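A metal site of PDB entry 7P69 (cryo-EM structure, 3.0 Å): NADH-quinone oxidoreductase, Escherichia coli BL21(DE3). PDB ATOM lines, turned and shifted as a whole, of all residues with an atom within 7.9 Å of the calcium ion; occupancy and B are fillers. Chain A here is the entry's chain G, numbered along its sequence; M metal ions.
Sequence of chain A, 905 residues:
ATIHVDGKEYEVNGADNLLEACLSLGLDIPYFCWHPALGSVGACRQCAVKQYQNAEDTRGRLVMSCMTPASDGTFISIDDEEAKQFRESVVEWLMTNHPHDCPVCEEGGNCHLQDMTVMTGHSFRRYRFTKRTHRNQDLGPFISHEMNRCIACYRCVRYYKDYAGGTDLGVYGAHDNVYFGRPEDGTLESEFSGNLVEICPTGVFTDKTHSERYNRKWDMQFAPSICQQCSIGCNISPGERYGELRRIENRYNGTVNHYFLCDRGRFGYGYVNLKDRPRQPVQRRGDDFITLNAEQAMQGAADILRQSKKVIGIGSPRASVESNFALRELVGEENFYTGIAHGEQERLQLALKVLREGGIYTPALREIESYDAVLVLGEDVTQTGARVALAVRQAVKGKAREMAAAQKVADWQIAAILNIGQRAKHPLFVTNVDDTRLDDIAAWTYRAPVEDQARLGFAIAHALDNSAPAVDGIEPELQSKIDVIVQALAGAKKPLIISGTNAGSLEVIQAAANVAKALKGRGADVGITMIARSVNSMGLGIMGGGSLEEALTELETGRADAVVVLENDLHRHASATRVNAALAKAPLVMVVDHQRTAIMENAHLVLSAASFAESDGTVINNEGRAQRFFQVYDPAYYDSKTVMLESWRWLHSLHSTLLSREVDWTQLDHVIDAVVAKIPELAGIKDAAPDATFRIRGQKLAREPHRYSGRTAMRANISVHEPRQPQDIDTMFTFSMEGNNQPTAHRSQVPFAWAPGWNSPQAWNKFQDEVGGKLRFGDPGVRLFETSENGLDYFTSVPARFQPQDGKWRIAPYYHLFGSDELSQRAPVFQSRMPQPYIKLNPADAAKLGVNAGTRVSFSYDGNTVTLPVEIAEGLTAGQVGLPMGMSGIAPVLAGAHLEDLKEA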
ATOM      1  N   GLU A 614      20.953 -27.892   7.685  1.00  0.00           N
ATOM      2  CA  GLU A 614      21.123 -27.560   6.275  1.00  0.00           C
ATOM      3  C   GLU A 614      20.848 -28.740   5.352  1.00  0.00           C
ATOM      4  O   GLU A 614      21.263 -28.711   4.190  1.00  0.00           O
ATOM      5  CB  GLU A 614      22.525 -27.011   6.029  1.00  0.00           C
ATOM      6  CG  GLU A 614      22.902 -25.869   6.925  1.00  0.00           C
ATOM      7  CD  GLU A 614      23.912 -26.248   7.967  1.00  0.00           C
ATOM      8  OE1 GLU A 614      24.358 -27.417   7.971  1.00  0.00           O
ATOM      9  OE2 GLU A 614      24.275 -25.393   8.787  1.00  0.00           O
ATOM     10  N   SER A 615      20.165 -29.770   5.832  1.00  0.00           N
ATOM     11  CA  SER A 615      19.940 -30.957   5.022  1.00  0.00           C
ATOM     12  C   SER A 615      18.561 -31.537   5.282  1.00  0.00           C
ATOM     13  O   SER A 615      17.932 -31.276   6.303  1.00  0.00           O
ATOM     14  CB  SER A 615      21.003 -32.027   5.292  1.00  0.00           C
ATOM     15  OG  SER A 615      21.051 -32.378   6.655  1.00  0.00           O
ATOM     16  N   ASP A 616      18.105 -32.331   4.326  1.00  0.00           N
ATOM     17  CA  ASP A 616      16.926 -33.159   4.447  1.00  0.00           C
ATOM     18  C   ASP A 616      17.356 -34.607   4.588  1.00  0.00           C
ATOM     19  O   ASP A 616      18.457 -34.984   4.202  1.00  0.00           O
ATOM     20  CB  ASP A 616      16.011 -33.006   3.239  1.00  0.00           C
ATOM     21  CG  ASP A 616      15.941 -31.592   2.745  1.00  0.00           C
ATOM     22  OD1 ASP A 616      15.236 -30.778   3.377  1.00  0.00           O
ATOM     23  OD2 ASP A 616      16.594 -31.294   1.734  1.00  0.00           O
ATOM     24  N   GLY A 617      16.476 -35.426   5.139  1.00  0.00           N
ATOM     25  CA  GLY A 617      16.771 -36.840   5.219  1.00  0.00           C
ATOM     26  C   GLY A 617      15.767 -37.554   6.082  1.00  0.00           C
ATOM     27  O   GLY A 617      14.782 -36.986   6.555  1.00  0.00           O
ATOM     28  N   PHE A 630      13.638 -31.887   7.656  1.00  0.00           N
ATOM     29  CA  PHE A 630      13.665 -30.989   6.518  1.00  0.00           C
ATOM     30  C   PHE A 630      14.705 -29.921   6.764  1.00  0.00           C
ATOM     31  O   PHE A 630      15.030 -29.593   7.902  1.00  0.00           O
ATOM     32  CB  PHE A 630      12.283 -30.365   6.288  1.00  0.00           C
ATOM     33  CG  PHE A 630      11.184 -31.360   6.039  1.00  0.00           C
ATOM     34  CD1 PHE A 630      10.553 -32.010   7.081  1.00  0.00           C
ATOM     35  CD2 PHE A 630      10.785 -31.647   4.760  1.00  0.00           C
ATOM     36  CE1 PHE A 630       9.554 -32.922   6.849  1.00  0.00           C
ATOM     37  CE2 PHE A 630       9.785 -32.557   4.514  1.00  0.00           C
ATOM     38  CZ  PHE A 630       9.169 -33.194   5.559  1.00  0.00           C
ATOM     39  N   GLN A 631      15.260 -29.391   5.674  1.00  0.00           N
ATOM     40  CA  GLN A 631      16.290 -28.377   5.769  1.00  0.00           C
ATOM     41  C   GLN A 631      15.720 -27.073   6.319  1.00  0.00           C
ATOM     42  O   GLN A 631      14.620 -26.655   5.951  1.00  0.00           O
ATOM     43  CB  GLN A 631      16.921 -28.156   4.406  1.00  0.00           C
ATOM     44  CG  GLN A 631      17.896 -27.036   4.318  1.00  0.00           C
ATOM     45  CD  GLN A 631      18.614 -27.026   2.996  1.00  0.00           C
ATOM     46  OE1 GLN A 631      18.426 -27.924   2.189  1.00  0.00           O
ATOM     47  NE2 GLN A 631      19.428 -26.015   2.763  1.00  0.00           N
ATOM     48  N   VAL A 632      16.467 -26.431   7.214  1.00  0.00           N
ATOM     49  CA  VAL A 632      15.992 -25.192   7.818  1.00  0.00           C
ATOM     50  C   VAL A 632      16.318 -24.007   6.928  1.00  0.00           C
ATOM     51  O   VAL A 632      15.464 -23.139   6.698  1.00  0.00           O
ATOM     52  CB  VAL A 632      16.575 -25.026   9.222  1.00  0.00           C
ATOM     53  CG1 VAL A 632      15.955 -23.836   9.927  1.00  0.00           C
ATOM     54  CG2 VAL A 632      16.357 -26.277  10.027  1.00  0.00           C
ATOM     55  N   TYR A 633      17.544 -23.938   6.412  1.00  0.00           N
ATOM     56  CA  TYR A 633      17.979 -22.762   5.692  1.00  0.00           C
ATOM     57  C   TYR A 633      18.991 -23.151   4.636  1.00  0.00           C
ATOM     58  O   TYR A 633      19.605 -24.214   4.682  1.00  0.00           O
ATOM     59  CB  TYR A 633      18.593 -21.713   6.631  1.00  0.00           C
ATOM     60  CG  TYR A 633      19.836 -22.169   7.356  1.00  0.00           C
ATOM     61  CD1 TYR A 633      19.756 -22.985   8.479  1.00  0.00           C
ATOM     62  CD2 TYR A 633      21.102 -21.784   6.929  1.00  0.00           C
ATOM     63  CE1 TYR A 633      20.872 -23.402   9.145  1.00  0.00           C
ATOM     64  CE2 TYR A 633      22.229 -22.199   7.588  1.00  0.00           C
ATOM     65  CZ  TYR A 633      22.103 -23.002   8.694  1.00  0.00           C
ATOM     66  OH  TYR A 633      23.224 -23.426   9.365  1.00  0.00           O
ATOM     67  N   ASP A 634      19.163 -22.242   3.678  1.00  0.00           N
ATOM     68  CA  ASP A 634      20.201 -22.385   2.673  1.00  0.00           C
ATOM     69  C   ASP A 634      21.491 -21.777   3.201  1.00  0.00           C
ATOM     70  O   ASP A 634      21.511 -20.595   3.543  1.00  0.00           O
ATOM     71  CB  ASP A 634      19.790 -21.701   1.388  1.00  0.00           C
ATOM     72  CG  ASP A 634      20.752 -21.933   0.262  1.00  0.00           C
ATOM     73  OD1 ASP A 634      21.089 -23.107   0.005  1.00  0.00           O
ATOM     74  OD2 ASP A 634      21.183 -20.947  -0.366  1.00  0.00           O
ATOM     75  N   PRO A 635      22.581 -22.542   3.304  1.00  0.00           N
ATOM     76  CA  PRO A 635      23.818 -21.984   3.851  1.00  0.00           C
ATOM     77  C   PRO A 635      24.486 -20.972   2.924  1.00  0.00           C
ATOM     78  O   PRO A 635      25.279 -20.161   3.407  1.00  0.00           O
ATOM     79  CB  PRO A 635      24.710 -23.213   4.052  1.00  0.00           C
ATOM     80  CG  PRO A 635      23.859 -24.394   3.772  1.00  0.00           C
ATOM     81  CD  PRO A 635      22.732 -23.957   2.923  1.00  0.00           C
ATOM     82  N   MET A 644      28.026 -26.303   0.755  1.00  0.00           N
ATOM     83  CA  MET A 644      27.687 -27.195   1.861  1.00  0.00           C
ATOM     84  C   MET A 644      26.458 -27.993   1.423  1.00  0.00           C
ATOM     85  O   MET A 644      25.319 -27.567   1.648  1.00  0.00           O
ATOM     86  CB  MET A 644      27.431 -26.425   3.145  1.00  0.00           C
ATOM     87  CG  MET A 644      28.412 -26.749   4.244  1.00  0.00           C
ATOM     88  SD  MET A 644      28.538 -25.449   5.484  1.00  0.00           S
ATOM     89  CE  MET A 644      26.869 -25.448   6.125  1.00  0.00           C
ATOM     90  N   LEU A 645      26.698 -29.133   0.799  1.00  0.00           N
ATOM     91  CA  LEU A 645      25.634 -29.950   0.250  1.00  0.00           C
ATOM     92  C   LEU A 645      25.288 -31.073   1.199  1.00  0.00           C
ATOM     93  O   LEU A 645      26.025 -31.385   2.142  1.00  0.00           O
ATOM     94  CB  LEU A 645      26.056 -30.509  -1.112  1.00  0.00           C
ATOM     95  CG  LEU A 645      26.555 -29.454  -2.096  1.00  0.00           C
ATOM     96  CD1 LEU A 645      26.968 -30.099  -3.377  1.00  0.00           C
ATOM     97  CD2 LEU A 645      25.486 -28.414  -2.344  1.00  0.00           C
ATOM     98  N   GLU A 646      24.131 -31.680   0.958  1.00  0.00           N
ATOM     99  CA  GLU A 646      23.735 -32.874   1.694  1.00  0.00           C
ATOM    100  C   GLU A 646      24.704 -34.015   1.390  1.00  0.00           C
ATOM    101  O   GLU A 646      25.296 -34.074   0.310  1.00  0.00           O
ATOM    102  CB  GLU A 646      22.311 -33.274   1.344  1.00  0.00           C
ATOM    103  CG  GLU A 646      21.250 -32.255   1.701  1.00  0.00           C
ATOM    104  CD  GLU A 646      21.031 -31.196   0.631  1.00  0.00           C
ATOM    105  OE1 GLU A 646      21.755 -31.209  -0.377  1.00  0.00           O
ATOM    106  OE2 GLU A 646      20.131 -30.353   0.810  1.00  0.00           O
ATOM    107  N   TRP A 648      24.064 -37.234   1.007  1.00  0.00           N
ATOM    108  CA  TRP A 648      23.555 -38.046  -0.089  1.00  0.00           C
ATOM    109  C   TRP A 648      23.728 -37.350  -1.426  1.00  0.00           C
ATOM    110  O   TRP A 648      23.970 -38.014  -2.437  1.00  0.00           O
ATOM    111  CB  TRP A 648      22.085 -38.414   0.151  1.00  0.00           C
ATOM    112  CG  TRP A 648      21.201 -37.258   0.493  1.00  0.00           C
ATOM    113  CD1 TRP A 648      20.875 -36.822   1.728  1.00  0.00           C
ATOM    114  CD2 TRP A 648      20.513 -36.404  -0.430  1.00  0.00           C
ATOM    115  NE1 TRP A 648      20.026 -35.749   1.641  1.00  0.00           N
ATOM    116  CE2 TRP A 648      19.796 -35.472   0.325  1.00  0.00           C
ATOM    117  CE3 TRP A 648      20.444 -36.339  -1.824  1.00  0.00           C
ATOM    118  CZ2 TRP A 648      19.019 -34.481  -0.257  1.00  0.00           C
ATOM    119  CZ3 TRP A 648      19.680 -35.367  -2.403  1.00  0.00           C
ATOM    120  CH2 TRP A 648      18.980 -34.445  -1.622  1.00  0.00           C
ATOM    121  N   ARG A 649      23.637 -36.020  -1.460  1.00  0.00           N
ATOM    122  CA  ARG A 649      23.865 -35.283  -2.701  1.00  0.00           C
ATOM    123  C   ARG A 649      25.327 -35.375  -3.133  1.00  0.00           C
ATOM    124  O   ARG A 649      25.614 -35.632  -4.309  1.00  0.00           O
ATOM    125  CB  ARG A 649      23.418 -33.830  -2.527  1.00  0.00           C
ATOM    126  CG  ARG A 649      23.810 -32.930  -3.669  1.00  0.00           C
ATOM    127  CD  ARG A 649      22.912 -31.718  -3.758  1.00  0.00           C
ATOM    128  NE  ARG A 649      21.609 -32.032  -4.324  1.00  0.00           N
ATOM    129  CZ  ARG A 649      20.451 -31.818  -3.728  1.00  0.00           C
ATOM    130  NH1 ARG A 649      20.376 -31.268  -2.531  1.00  0.00           N
ATOM    131  NH2 ARG A 649      19.321 -32.158  -4.349  1.00  0.00           N
ATOM    132  N   LEU A 668      15.997 -35.359  -3.467  1.00  0.00           N
ATOM    133  CA  LEU A 668      15.835 -36.210  -2.298  1.00  0.00           C
ATOM    134  C   LEU A 668      14.868 -37.362  -2.567  1.00  0.00           C
ATOM    135  O   LEU A 668      15.094 -38.494  -2.126  1.00  0.00           O
ATOM    136  CB  LEU A 668      15.345 -35.392  -1.097  1.00  0.00           C
ATOM    137  CG  LEU A 668      14.999 -36.179   0.165  1.00  0.00           C
ATOM    138  CD1 LEU A 668      16.245 -36.697   0.846  1.00  0.00           C
ATOM    139  CD2 LEU A 668      14.150 -35.363   1.108  1.00  0.00           C
ATOM    140  N   ARG A 703       8.251 -21.900   5.399  1.00  0.00           N
ATOM    141  CA  ARG A 703       9.214 -22.054   6.475  1.00  0.00           C
ATOM    142  C   ARG A 703       9.196 -20.890   7.446  1.00  0.00           C
ATOM    143  O   ARG A 703       9.539 -21.071   8.622  1.00  0.00           O
ATOM    144  CB  ARG A 703      10.622 -22.214   5.912  1.00  0.00           C
ATOM    145  CG  ARG A 703      10.990 -23.624   5.533  1.00  0.00           C
ATOM    146  CD  ARG A 703      12.418 -23.705   5.091  1.00  0.00           C
ATOM    147  NE  ARG A 703      12.820 -25.076   4.786  1.00  0.00           N
ATOM    148  CZ  ARG A 703      12.775 -25.623   3.586  1.00  0.00           C
ATOM    149  NH1 ARG A 703      12.359 -24.947   2.532  1.00  0.00           N
ATOM    150  NH2 ARG A 703      13.154 -26.885   3.438  1.00  0.00           N
ATOM    151  N   GLN A 727      15.700 -21.873  -3.883  1.00  0.00           N
ATOM    152  CA  GLN A 727      14.687 -22.802  -4.344  1.00  0.00           C
ATOM    153  C   GLN A 727      14.910 -24.160  -3.710  1.00  0.00           C
ATOM    154  O   GLN A 727      16.034 -24.667  -3.677  1.00  0.00           O
ATOM    155  CB  GLN A 727      14.721 -22.917  -5.872  1.00  0.00           C
ATOM    156  CG  GLN A 727      14.300 -21.639  -6.563  1.00  0.00           C
ATOM    157  CD  GLN A 727      12.911 -21.200  -6.160  1.00  0.00           C
ATOM    158  OE1 GLN A 727      12.732 -20.193  -5.483  1.00  0.00           O
ATOM    159  NE2 GLN A 727      11.904 -21.953  -6.586  1.00  0.00           N
ATOM    160  N   ASP A 728      13.841 -24.732  -3.159  1.00  0.00           N
ATOM    161  CA  ASP A 728      13.884 -26.044  -2.530  1.00  0.00           C
ATOM    162  C   ASP A 728      13.273 -27.047  -3.487  1.00  0.00           C
ATOM    163  O   ASP A 728      12.048 -27.109  -3.639  1.00  0.00           O
ATOM    164  CB  ASP A 728      13.146 -26.016  -1.198  1.00  0.00           C
ATOM    165  CG  ASP A 728      13.404 -27.234  -0.364  1.00  0.00           C
ATOM    166  OD1 ASP A 728      14.586 -27.627  -0.218  1.00  0.00           O
ATOM    167  OD2 ASP A 728      12.434 -27.808   0.154  1.00  0.00           O
ATOM    168  N   ILE A 729      14.121 -27.855  -4.144  1.00  0.00           N
ATOM    169  CA  ILE A 729      13.621 -28.901  -5.013  1.00  0.00           C
ATOM    170  C   ILE A 729      13.444 -30.220  -4.277  1.00  0.00           C
ATOM    171  O   ILE A 729      12.777 -31.128  -4.810  1.00  0.00           O
ATOM    172  CB  ILE A 729      14.548 -29.122  -6.223  1.00  0.00           C
ATOM    173  CG1 ILE A 729      15.930 -29.567  -5.768  1.00  0.00           C
ATOM    174  CG2 ILE A 729      14.658 -27.846  -7.047  1.00  0.00           C
ATOM    175  CD1 ILE A 729      16.822 -30.033  -6.890  1.00  0.00           C
ATOM    176  N   ASP A 730      13.984 -30.344  -3.072  1.00  0.00           N
ATOM    177  CA  ASP A 730      13.972 -31.632  -2.385  1.00  0.00           C
ATOM    178  C   ASP A 730      12.648 -31.876  -1.675  1.00  0.00           C
ATOM    179  O   ASP A 730      12.161 -33.009  -1.641  1.00  0.00           O
ATOM    180  CB  ASP A 730      15.119 -31.692  -1.387  1.00  0.00           C
ATOM    181  CG  ASP A 730      16.460 -31.653  -2.059  1.00  0.00           C
ATOM    182  OD1 ASP A 730      16.585 -32.168  -3.183  1.00  0.00           O
ATOM    183  OD2 ASP A 730      17.403 -31.096  -1.459  1.00  0.00           O
ATOM    184  N   THR A 731      12.069 -30.845  -1.060  1.00  0.00           N
ATOM    185  CA  THR A 731      10.921 -31.018  -0.193  1.00  0.00           C
ATOM    186  C   THR A 731       9.786 -30.098  -0.628  1.00  0.00           C
ATOM    187  O   THR A 731       9.932 -29.265  -1.531  1.00  0.00           O
ATOM    188  CB  THR A 731      11.254 -30.752   1.279  1.00  0.00           C
ATOM    189  OG1 THR A 731      11.471 -29.354   1.485  1.00  0.00           O
ATOM    190  CG2 THR A 731      12.506 -31.508   1.692  1.00  0.00           C
ATOM    191  N   PHE A 735      11.562 -21.750   0.931  1.00  0.00           N
ATOM    192  CA  PHE A 735      12.419 -20.871   1.720  1.00  0.00           C
ATOM    193  C   PHE A 735      11.890 -19.445   1.730  1.00  0.00           C
ATOM    194  O   PHE A 735      12.602 -18.496   1.397  1.00  0.00           O
ATOM    195  CB  PHE A 735      13.851 -20.909   1.201  1.00  0.00           C
ATOM    196  CG  PHE A 735      14.579 -22.185   1.519  1.00  0.00           C
ATOM    197  CD1 PHE A 735      14.981 -22.461   2.815  1.00  0.00           C
ATOM    198  CD2 PHE A 735      14.889 -23.080   0.523  1.00  0.00           C
ATOM    199  CE1 PHE A 735      15.659 -23.621   3.105  1.00  0.00           C
ATOM    200  CE2 PHE A 735      15.560 -24.246   0.812  1.00  0.00           C
ATOM    201  CZ  PHE A 735      15.944 -24.515   2.096  1.00  0.00           C
HETATM  202 CA    CA M   1      17.812 -29.524   0.426  1.00  0.00          CA
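The calcium ion is bound by the side-chain amide oxygen (OE1) of Gln 631 (2.5 Å), the side-chain carboxylate (OD2) of Asp 730 (2.5 Å), the side-chain carboxylate (OE2) of Glu 646 (2.5 Å) and the side-chain carboxylate (OD2) of Asp 616 (2.5 Å).
Asp 728 touches the calcium ion (OD1 to CA, 3.8 Å).
Of the 23 residues printed, 5 come within 4 Å of the calcium ion.
The nearest printed residue that does not touch the calcium ion is Arg 649 (4.3 Å).
NH2 of Arg 703 is in salt-bridge range of OD2 of Asp 728 (3.5 Å).
O of Gln 631 lies within hydrogen-bond range of NE of Arg 703, 2.7 Å away.
NH1 of Arg 649 is in salt-bridge range of OE1 of Glu 646, 2.6 Å away.
The side-chain amide nitrogen (NE2) of Gln 631 is in hydrogen-bond range of the backbone carbonyl oxygen (O) of Tyr 633, at 2.6 Å.
The backbone NH (N) of Gln 631 lies within hydrogen-bond range of the backbone carbonyl oxygen (O) of Ser 615.
The side-chain carboxylate of Asp 730 is in salt-bridge range of the guanidinium group of Arg 649 (3.0 Å).
The backbone NH of Leu 668 is in hydrogen-bond range of the side-chain carboxylate of Asp 730, 3.3 Å away.
NE1 of Trp 648 lies within hydrogen-bond range of O of Asp 616 (3.1 Å).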
